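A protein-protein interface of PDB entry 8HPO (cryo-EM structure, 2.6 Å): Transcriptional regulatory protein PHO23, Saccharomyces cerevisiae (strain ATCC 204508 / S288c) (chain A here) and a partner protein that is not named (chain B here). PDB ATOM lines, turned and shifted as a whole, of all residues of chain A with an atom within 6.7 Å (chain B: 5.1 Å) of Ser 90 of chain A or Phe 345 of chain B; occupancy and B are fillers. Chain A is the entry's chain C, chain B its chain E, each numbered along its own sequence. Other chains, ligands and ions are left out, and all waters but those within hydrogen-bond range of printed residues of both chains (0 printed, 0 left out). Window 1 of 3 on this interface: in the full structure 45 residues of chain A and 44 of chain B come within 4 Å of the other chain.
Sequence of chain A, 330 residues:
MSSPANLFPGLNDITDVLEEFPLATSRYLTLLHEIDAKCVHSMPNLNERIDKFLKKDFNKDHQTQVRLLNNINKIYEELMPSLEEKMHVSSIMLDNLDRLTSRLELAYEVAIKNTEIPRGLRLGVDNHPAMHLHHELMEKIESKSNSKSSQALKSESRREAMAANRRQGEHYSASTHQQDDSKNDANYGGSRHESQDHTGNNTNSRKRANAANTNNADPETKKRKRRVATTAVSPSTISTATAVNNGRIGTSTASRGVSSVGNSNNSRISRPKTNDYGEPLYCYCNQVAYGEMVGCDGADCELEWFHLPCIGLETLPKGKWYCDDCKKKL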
ATOM      1  N   LEU A  32     -32.319 -14.032  15.403  1.00  0.00           N
ATOM      2  CA  LEU A  32     -33.094 -12.810  15.222  1.00  0.00           C
ATOM      3  C   LEU A  32     -34.511 -12.969  15.756  1.00  0.00           C
ATOM      4  O   LEU A  32     -35.029 -12.072  16.428  1.00  0.00           O
ATOM      5  CB  LEU A  32     -33.115 -12.416  13.749  1.00  0.00           C
ATOM      6  CG  LEU A  32     -31.781 -11.983  13.148  1.00  0.00           C
ATOM      7  CD1 LEU A  32     -31.979 -11.455  11.754  1.00  0.00           C
ATOM      8  CD2 LEU A  32     -31.116 -10.943  14.018  1.00  0.00           C
ATOM      9  N   ASP A  36     -36.283 -10.629  18.679  1.00  0.00           N
ATOM     10  CA  ASP A  36     -37.601 -10.018  18.520  1.00  0.00           C
ATOM     11  C   ASP A  36     -38.503 -10.210  19.729  1.00  0.00           C
ATOM     12  O   ASP A  36     -39.176  -9.263  20.138  1.00  0.00           O
ATOM     13  CB  ASP A  36     -38.319 -10.594  17.303  1.00  0.00           C
ATOM     14  CG  ASP A  36     -37.848  -9.995  16.009  1.00  0.00           C
ATOM     15  OD1 ASP A  36     -36.942  -9.140  16.044  1.00  0.00           O
ATOM     16  OD2 ASP A  36     -38.386 -10.380  14.952  1.00  0.00           O
ATOM     17  N   LEU A  83     -31.404  -3.290  20.222  1.00  0.00           N
ATOM     18  CA  LEU A  83     -31.118  -2.864  18.857  1.00  0.00           C
ATOM     19  C   LEU A  83     -29.651  -3.008  18.482  1.00  0.00           C
ATOM     20  O   LEU A  83     -29.318  -2.836  17.307  1.00  0.00           O
ATOM     21  CB  LEU A  83     -31.550  -1.415  18.645  1.00  0.00           C
ATOM     22  CG  LEU A  83     -33.043  -1.101  18.739  1.00  0.00           C
ATOM     23  CD1 LEU A  83     -33.322   0.278  18.167  1.00  0.00           C
ATOM     24  CD2 LEU A  83     -33.868  -2.145  18.023  1.00  0.00           C
ATOM     25  N   GLU A  85     -27.943  -5.921  19.585  1.00  0.00           N
ATOM     26  CA  GLU A  85     -27.977  -7.352  19.313  1.00  0.00           C
ATOM     27  C   GLU A  85     -28.251  -7.620  17.840  1.00  0.00           C
ATOM     28  O   GLU A  85     -27.554  -8.411  17.193  1.00  0.00           O
ATOM     29  CB  GLU A  85     -29.049  -8.024  20.171  1.00  0.00           C
ATOM     30  CG  GLU A  85     -28.543  -8.688  21.428  1.00  0.00           C
ATOM     31  CD  GLU A  85     -28.553  -7.758  22.618  1.00  0.00           C
ATOM     32  OE1 GLU A  85     -28.529  -6.532  22.411  1.00  0.00           O
ATOM     33  OE2 GLU A  85     -28.592  -8.251  23.763  1.00  0.00           O
ATOM     34  N   LYS A  86     -29.301  -6.992  17.309  1.00  0.00           N
ATOM     35  CA  LYS A  86     -29.702  -7.216  15.928  1.00  0.00           C
ATOM     36  C   LYS A  86     -28.566  -6.960  14.951  1.00  0.00           C
ATOM     37  O   LYS A  86     -28.296  -7.781  14.069  1.00  0.00           O
ATOM     38  CB  LYS A  86     -30.902  -6.336  15.590  1.00  0.00           C
ATOM     39  CG  LYS A  86     -32.189  -6.775  16.236  1.00  0.00           C
ATOM     40  CD  LYS A  86     -33.354  -6.026  15.629  1.00  0.00           C
ATOM     41  CE  LYS A  86     -34.672  -6.440  16.252  1.00  0.00           C
ATOM     42  NZ  LYS A  86     -34.949  -5.707  17.513  1.00  0.00           N
ATOM     43  N   MET A  87     -27.881  -5.829  15.087  1.00  0.00           N
ATOM     44  CA  MET A  87     -26.862  -5.520  14.096  1.00  0.00           C
ATOM     45  C   MET A  87     -25.577  -6.304  14.330  1.00  0.00           C
ATOM     46  O   MET A  87     -24.866  -6.605  13.366  1.00  0.00           O
ATOM     47  CB  MET A  87     -26.592  -4.018  14.048  1.00  0.00           C
ATOM     48  CG  MET A  87     -26.799  -3.271  15.336  1.00  0.00           C
ATOM     49  SD  MET A  87     -26.444  -1.526  15.086  1.00  0.00           S
ATOM     50  CE  MET A  87     -24.846  -1.625  14.300  1.00  0.00           C
ATOM     51  N   HIS A  88     -25.296  -6.715  15.567  1.00  0.00           N
ATOM     52  CA  HIS A  88     -24.194  -7.650  15.784  1.00  0.00           C
ATOM     53  C   HIS A  88     -24.442  -8.970  15.057  1.00  0.00           C
ATOM     54  O   HIS A  88     -23.576  -9.470  14.315  1.00  0.00           O
ATOM     55  CB  HIS A  88     -24.001  -7.882  17.282  1.00  0.00           C
ATOM     56  CG  HIS A  88     -22.764  -8.651  17.617  1.00  0.00           C
ATOM     57  ND1 HIS A  88     -22.774  -9.754  18.439  1.00  0.00           N
ATOM     58  CD2 HIS A  88     -21.479  -8.480  17.230  1.00  0.00           C
ATOM     59  CE1 HIS A  88     -21.548 -10.231  18.549  1.00  0.00           C
ATOM     60  NE2 HIS A  88     -20.742  -9.475  17.826  1.00  0.00           N
ATOM     61  N   VAL A  89     -25.629  -9.548  15.265  1.00  0.00           N
ATOM     62  CA  VAL A  89     -25.991 -10.803  14.609  1.00  0.00           C
ATOM     63  C   VAL A  89     -25.954 -10.647  13.096  1.00  0.00           C
ATOM     64  O   VAL A  89     -25.453 -11.522  12.379  1.00  0.00           O
ATOM     65  CB  VAL A  89     -27.371 -11.280  15.089  1.00  0.00           C
ATOM     66  CG1 VAL A  89     -27.729 -12.585  14.429  1.00  0.00           C
ATOM     67  CG2 VAL A  89     -27.374 -11.444  16.585  1.00  0.00           C
ATOM     68  N   SER A  90     -26.508  -9.548  12.583  1.00  0.00           N
ATOM     69  CA  SER A  90     -26.474  -9.303  11.149  1.00  0.00           C
ATOM     70  C   SER A  90     -25.051  -9.209  10.620  1.00  0.00           C
ATOM     71  O   SER A  90     -24.781  -9.655   9.502  1.00  0.00           O
ATOM     72  CB  SER A  90     -27.241  -8.029  10.825  1.00  0.00           C
ATOM     73  OG  SER A  90     -28.615  -8.313  10.694  1.00  0.00           O
ATOM     74  N   SER A  91     -24.120  -8.674  11.410  1.00  0.00           N
ATOM     75  CA  SER A  91     -22.749  -8.555  10.924  1.00  0.00           C
ATOM     76  C   SER A  91     -22.062  -9.914  10.841  1.00  0.00           C
ATOM     77  O   SER A  91     -21.347 -10.201   9.867  1.00  0.00           O
ATOM     78  CB  SER A  91     -21.967  -7.610  11.824  1.00  0.00           C
ATOM     79  OG  SER A  91     -22.413  -7.739  13.157  1.00  0.00           O
ATOM     80  N   ILE A  92     -22.282 -10.779  11.833  1.00  0.00           N
ATOM     81  CA  ILE A  92     -21.648 -12.097  11.744  1.00  0.00           C
ATOM     82  C   ILE A  92     -22.292 -12.930  10.637  1.00  0.00           C
ATOM     83  O   ILE A  92     -21.599 -13.641   9.891  1.00  0.00           O
ATOM     84  CB  ILE A  92     -21.665 -12.826  13.100  1.00  0.00           C
ATOM     85  CG1 ILE A  92     -22.999 -12.658  13.810  1.00  0.00           C
ATOM     86  CG2 ILE A  92     -20.533 -12.334  13.975  1.00  0.00           C
ATOM     87  CD1 ILE A  92     -22.962 -13.098  15.245  1.00  0.00           C
ATOM     88  N   MET A  93     -23.622 -12.853  10.509  1.00  0.00           N
ATOM     89  CA  MET A  93     -24.319 -13.475   9.387  1.00  0.00           C
ATOM     90  C   MET A  93     -23.742 -13.021   8.051  1.00  0.00           C
ATOM     91  O   MET A  93     -23.523 -13.835   7.144  1.00  0.00           O
ATOM     92  CB  MET A  93     -25.804 -13.136   9.479  1.00  0.00           C
ATOM     93  CG  MET A  93     -26.711 -13.798   8.474  1.00  0.00           C
ATOM     94  SD  MET A  93     -28.427 -13.557   8.973  1.00  0.00           S
ATOM     95  CE  MET A  93     -29.299 -14.071   7.502  1.00  0.00           C
ATOM     96  N   LEU A  94     -23.484 -11.720   7.916  1.00  0.00           N
ATOM     97  CA  LEU A  94     -22.973 -11.185   6.664  1.00  0.00           C
ATOM     98  C   LEU A  94     -21.585 -11.731   6.363  1.00  0.00           C
ATOM     99  O   LEU A  94     -21.276 -12.070   5.215  1.00  0.00           O
ATOM    100  CB  LEU A  94     -22.972  -9.657   6.728  1.00  0.00           C
ATOM    101  CG  LEU A  94     -22.875  -8.868   5.427  1.00  0.00           C
ATOM    102  CD1 LEU A  94     -21.446  -8.711   4.961  1.00  0.00           C
ATOM    103  CD2 LEU A  94     -23.666  -9.596   4.378  1.00  0.00           C
ATOM    104  N   ASP A  95     -20.735 -11.838   7.384  1.00  0.00           N
ATOM    105  CA  ASP A  95     -19.384 -12.340   7.136  1.00  0.00           C
ATOM    106  C   ASP A  95     -19.409 -13.808   6.715  1.00  0.00           C
ATOM    107  O   ASP A  95     -18.701 -14.218   5.780  1.00  0.00           O
ATOM    108  CB  ASP A  95     -18.517 -12.143   8.373  1.00  0.00           C
ATOM    109  CG  ASP A  95     -17.082 -11.854   8.021  1.00  0.00           C
ATOM    110  OD1 ASP A  95     -16.728 -12.039   6.837  1.00  0.00           O
ATOM    111  OD2 ASP A  95     -16.308 -11.447   8.916  1.00  0.00           O
ATOM    112  N   MET B 200     -38.750  -9.103   6.360  1.00  0.00           N
ATOM    113  CA  MET B 200     -38.276  -8.438   7.573  1.00  0.00           C
ATOM    114  C   MET B 200     -37.700  -7.060   7.259  1.00  0.00           C
ATOM    115  O   MET B 200     -37.794  -6.134   8.081  1.00  0.00           O
ATOM    116  CB  MET B 200     -37.259  -9.319   8.299  1.00  0.00           C
ATOM    117  CG  MET B 200     -35.833  -9.212   7.811  1.00  0.00           C
ATOM    118  SD  MET B 200     -34.805 -10.565   8.408  1.00  0.00           S
ATOM    119  CE  MET B 200     -35.457 -10.788  10.057  1.00  0.00           C
ATOM    120  N   GLU B 204     -38.679  -3.462   9.198  1.00  0.00           N
ATOM    121  CA  GLU B 204     -37.641  -2.581   9.713  1.00  0.00           C
ATOM    122  C   GLU B 204     -37.659  -1.225   9.022  1.00  0.00           C
ATOM    123  O   GLU B 204     -37.309  -0.215   9.639  1.00  0.00           O
ATOM    124  CB  GLU B 204     -36.279  -3.247   9.575  1.00  0.00           C
ATOM    125  CG  GLU B 204     -36.107  -4.440  10.495  1.00  0.00           C
ATOM    126  CD  GLU B 204     -36.548  -4.147  11.920  1.00  0.00           C
ATOM    127  OE1 GLU B 204     -37.350  -4.926  12.473  1.00  0.00           O
ATOM    128  OE2 GLU B 204     -36.089  -3.136  12.489  1.00  0.00           O
ATOM    129  N   ARG B 341     -28.921   2.971  14.122  1.00  0.00           N
ATOM    130  CA  ARG B 341     -28.769   1.532  14.312  1.00  0.00           C
ATOM    131  C   ARG B 341     -29.701   0.740  13.397  1.00  0.00           C
ATOM    132  O   ARG B 341     -29.280  -0.254  12.787  1.00  0.00           O
ATOM    133  CB  ARG B 341     -29.008   1.171  15.773  1.00  0.00           C
ATOM    134  CG  ARG B 341     -27.797   1.383  16.647  1.00  0.00           C
ATOM    135  CD  ARG B 341     -28.138   1.183  18.101  1.00  0.00           C
ATOM    136  NE  ARG B 341     -27.022   1.535  18.963  1.00  0.00           N
ATOM    137  CZ  ARG B 341     -27.023   1.375  20.279  1.00  0.00           C
ATOM    138  NH1 ARG B 341     -28.081   0.860  20.885  1.00  0.00           N
ATOM    139  NH2 ARG B 341     -25.964   1.727  20.988  1.00  0.00           N
ATOM    140  N   ASN B 342     -30.970   1.156  13.290  1.00  0.00           N
ATOM    141  CA  ASN B 342     -31.880   0.464  12.375  1.00  0.00           C
ATOM    142  C   ASN B 342     -31.402   0.558  10.933  1.00  0.00           C
ATOM    143  O   ASN B 342     -31.553  -0.391  10.152  1.00  0.00           O
ATOM    144  CB  ASN B 342     -33.291   1.024  12.501  1.00  0.00           C
ATOM    145  CG  ASN B 342     -34.008   0.506  13.713  1.00  0.00           C
ATOM    146  OD1 ASN B 342     -33.381   0.086  14.682  1.00  0.00           O
ATOM    147  ND2 ASN B 342     -35.330   0.526  13.672  1.00  0.00           N
ATOM    148  N   LYS B 343     -30.812   1.690  10.560  1.00  0.00           N
ATOM    149  CA  LYS B 343     -30.322   1.826   9.193  1.00  0.00           C
ATOM    150  C   LYS B 343     -29.167   0.870   8.916  1.00  0.00           C
ATOM    151  O   LYS B 343     -29.090   0.274   7.831  1.00  0.00           O
ATOM    152  CB  LYS B 343     -29.917   3.274   8.932  1.00  0.00           C
ATOM    153  CG  LYS B 343     -31.096   4.200   8.689  1.00  0.00           C
ATOM    154  CD  LYS B 343     -30.739   5.269   7.680  1.00  0.00           C
ATOM    155  CE  LYS B 343     -31.959   6.003   7.171  1.00  0.00           C
ATOM    156  NZ  LYS B 343     -31.628   6.870   6.008  1.00  0.00           N
ATOM    157  N   GLU B 344     -28.274   0.679   9.892  1.00  0.00           N
ATOM    158  CA  GLU B 344     -27.194  -0.286   9.683  1.00  0.00           C
ATOM    159  C   GLU B 344     -27.728  -1.714   9.590  1.00  0.00           C
ATOM    160  O   GLU B 344     -27.271  -2.503   8.748  1.00  0.00           O
ATOM    161  CB  GLU B 344     -26.159  -0.174  10.794  1.00  0.00           C
ATOM    162  CG  GLU B 344     -24.864  -0.887  10.481  1.00  0.00           C
ATOM    163  CD  GLU B 344     -24.173  -0.320   9.262  1.00  0.00           C
ATOM    164  OE1 GLU B 344     -24.323   0.889   9.000  1.00  0.00           O
ATOM    165  OE2 GLU B 344     -23.474  -1.083   8.564  1.00  0.00           O
ATOM    166  N   PHE B 345     -28.679  -2.065  10.462  1.00  0.00           N
ATOM    167  CA  PHE B 345     -29.389  -3.338  10.346  1.00  0.00           C
ATOM    168  C   PHE B 345     -29.886  -3.585   8.925  1.00  0.00           C
ATOM    169  O   PHE B 345     -29.647  -4.652   8.343  1.00  0.00           O
ATOM    170  CB  PHE B 345     -30.562  -3.358  11.323  1.00  0.00           C
ATOM    171  CG  PHE B 345     -31.214  -4.693  11.472  1.00  0.00           C
ATOM    172  CD1 PHE B 345     -32.576  -4.782  11.671  1.00  0.00           C
ATOM    173  CD2 PHE B 345     -30.479  -5.856  11.439  1.00  0.00           C
ATOM    174  CE1 PHE B 345     -33.190  -6.009  11.823  1.00  0.00           C
ATOM    175  CE2 PHE B 345     -31.094  -7.081  11.594  1.00  0.00           C
ATOM    176  CZ  PHE B 345     -32.445  -7.156  11.782  1.00  0.00           C
ATOM    177  N   ILE B 346     -30.597  -2.609   8.354  1.00  0.00           N
ATOM    178  CA  ILE B 346     -31.169  -2.806   7.025  1.00  0.00           C
ATOM    179  C   ILE B 346     -30.075  -2.973   5.977  1.00  0.00           C
ATOM    180  O   ILE B 346     -30.197  -3.793   5.056  1.00  0.00           O
ATOM    181  CB  ILE B 346     -32.115  -1.651   6.664  1.00  0.00           C
ATOM    182  CG1 ILE B 346     -33.319  -1.646   7.587  1.00  0.00           C
ATOM    183  CG2 ILE B 346     -32.598  -1.784   5.239  1.00  0.00           C
ATOM    184  CD1 ILE B 346     -34.290  -0.576   7.256  1.00  0.00           C
ATOM    185  N   ARG B 347     -29.004  -2.187   6.075  1.00  0.00           N
ATOM    186  CA  ARG B 347     -27.934  -2.307   5.087  1.00  0.00           C
ATOM    187  C   ARG B 347     -27.327  -3.710   5.100  1.00  0.00           C
ATOM    188  O   ARG B 347     -27.080  -4.315   4.039  1.00  0.00           O
ATOM    189  CB  ARG B 347     -26.880  -1.237   5.355  1.00  0.00           C
ATOM    190  CG  ARG B 347     -25.818  -1.112   4.297  1.00  0.00           C
ATOM    191  CD  ARG B 347     -24.810  -0.058   4.685  1.00  0.00           C
ATOM    192  NE  ARG B 347     -23.758   0.100   3.689  1.00  0.00           N
ATOM    193  CZ  ARG B 347     -22.503   0.419   3.985  1.00  0.00           C
ATOM    194  NH1 ARG B 347     -22.147   0.617   5.246  1.00  0.00           N
ATOM    195  NH2 ARG B 347     -21.603   0.543   3.022  1.00  0.00           N
ATOM    196  N   ASN B 348     -27.117  -4.260   6.298  1.00  0.00           N
ATOM    197  CA  ASN B 348     -26.635  -5.635   6.408  1.00  0.00           C
ATOM    198  C   ASN B 348     -27.607  -6.614   5.759  1.00  0.00           C
ATOM    199  O   ASN B 348     -27.203  -7.477   4.966  1.00  0.00           O
ATOM    200  CB  ASN B 348     -26.422  -6.007   7.872  1.00  0.00           C
ATOM    201  CG  ASN B 348     -25.159  -5.428   8.443  1.00  0.00           C
ATOM    202  OD1 ASN B 348     -24.183  -5.205   7.736  1.00  0.00           O
ATOM    203  ND2 ASN B 348     -25.173  -5.175   9.741  1.00  0.00           N
ATOM    204  N   LEU B 349     -28.891  -6.512   6.119  1.00  0.00           N
ATOM    205  CA  LEU B 349     -29.896  -7.419   5.570  1.00  0.00           C
ATOM    206  C   LEU B 349     -29.888  -7.413   4.046  1.00  0.00           C
ATOM    207  O   LEU B 349     -30.077  -8.458   3.408  1.00  0.00           O
ATOM    208  CB  LEU B 349     -31.277  -7.042   6.093  1.00  0.00           C
ATOM    209  CG  LEU B 349     -31.603  -7.561   7.486  1.00  0.00           C
ATOM    210  CD1 LEU B 349     -32.982  -7.109   7.884  1.00  0.00           C
ATOM    211  CD2 LEU B 349     -31.515  -9.066   7.514  1.00  0.00           C
ATOM    212  N   ILE B 352     -26.994  -9.405   2.676  1.00  0.00           N
ATOM    213  CA  ILE B 352     -27.297 -10.825   2.842  1.00  0.00           C
ATOM    214  C   ILE B 352     -28.202 -11.319   1.716  1.00  0.00           C
ATOM    215  O   ILE B 352     -27.898 -12.314   1.037  1.00  0.00           O
ATOM    216  CB  ILE B 352     -27.922 -11.075   4.226  1.00  0.00           C
ATOM    217  CG1 ILE B 352     -26.834 -11.124   5.295  1.00  0.00           C
ATOM    218  CG2 ILE B 352     -28.735 -12.348   4.230  1.00  0.00           C
ATOM    219  CD1 ILE B 352     -27.308 -10.715   6.650  1.00  0.00           C
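The backbone carbonyl oxygen (O) of Met 87 of chain A lies within hydrogen-bond range of the side-chain hydroxyl (OG) of Ser 91 of chain A. The side-chain hydroxyl (OG) of Ser 90 of chain A lies close to the backbone carbonyl oxygen (O) of Lys 86 of chain A, at 3.4 Å. The guanidinium group of Arg 347 of chain B is in salt-bridge range of the side-chain carboxylate of Glu 344 of chain B, at 3.96 Å.
Among the printed residues, pairs that only touch across the chains: Leu 32 of chain A with Met 200 of chain B, Leu 83 of chain A with Asn 342 of chain B, Lys 86 of chain A with Phe 345 of chain B, Met 87 of chain A with Arg 341 of chain B, Met 87 of chain A with Glu 344 of chain B, Met 87 of chain A with Asn 348 of chain B, Ser 90 of chain A with Phe 345 of chain B, Ser 90 of chain A with Asn 348 of chain B, Ser 90 of chain A with Ile 352 of chain B, Met 93 of chain A with Ile 352 of chain B and Leu 94 of chain A with Ile 352 of chain B.
Of chain A, only Lys 86 (3.8 Å) and Ser 90 (2.9 Å) come within 4 Å of Phe 345 of chain B. Of the printed residues of chain A, Glu 344 of chain B touches Met 87. Printed residues of chain B within 4 Å of Lys 86 of chain A: Phe 345. Lys 343 of chain B touches none of the printed residues of chain A. The nearest printed residue of chain B that does not touch Leu 32 of chain A is Phe 345 of chain B (4.3 Å).
Printed residues of chain B that touch a printed residue of chain A: Met 200, Arg 341, Asn 342, Glu 344, Phe 345, Asn 348 and Ile 352. Hydrophobic or aromatic side chains of chain B within 4 Å of the printed part of chain A: Met 200, Phe 345 and Ile 352. Along chain B the printed residues that touch a printed residue of chain A span positions 200 to 352. Among the printed residues, 11 pairs touch across the chains. Among the printed residues, no Asp or Glu carboxylate lies within 4 Å of a Lys or Arg side-chain nitrogen of the other chain.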
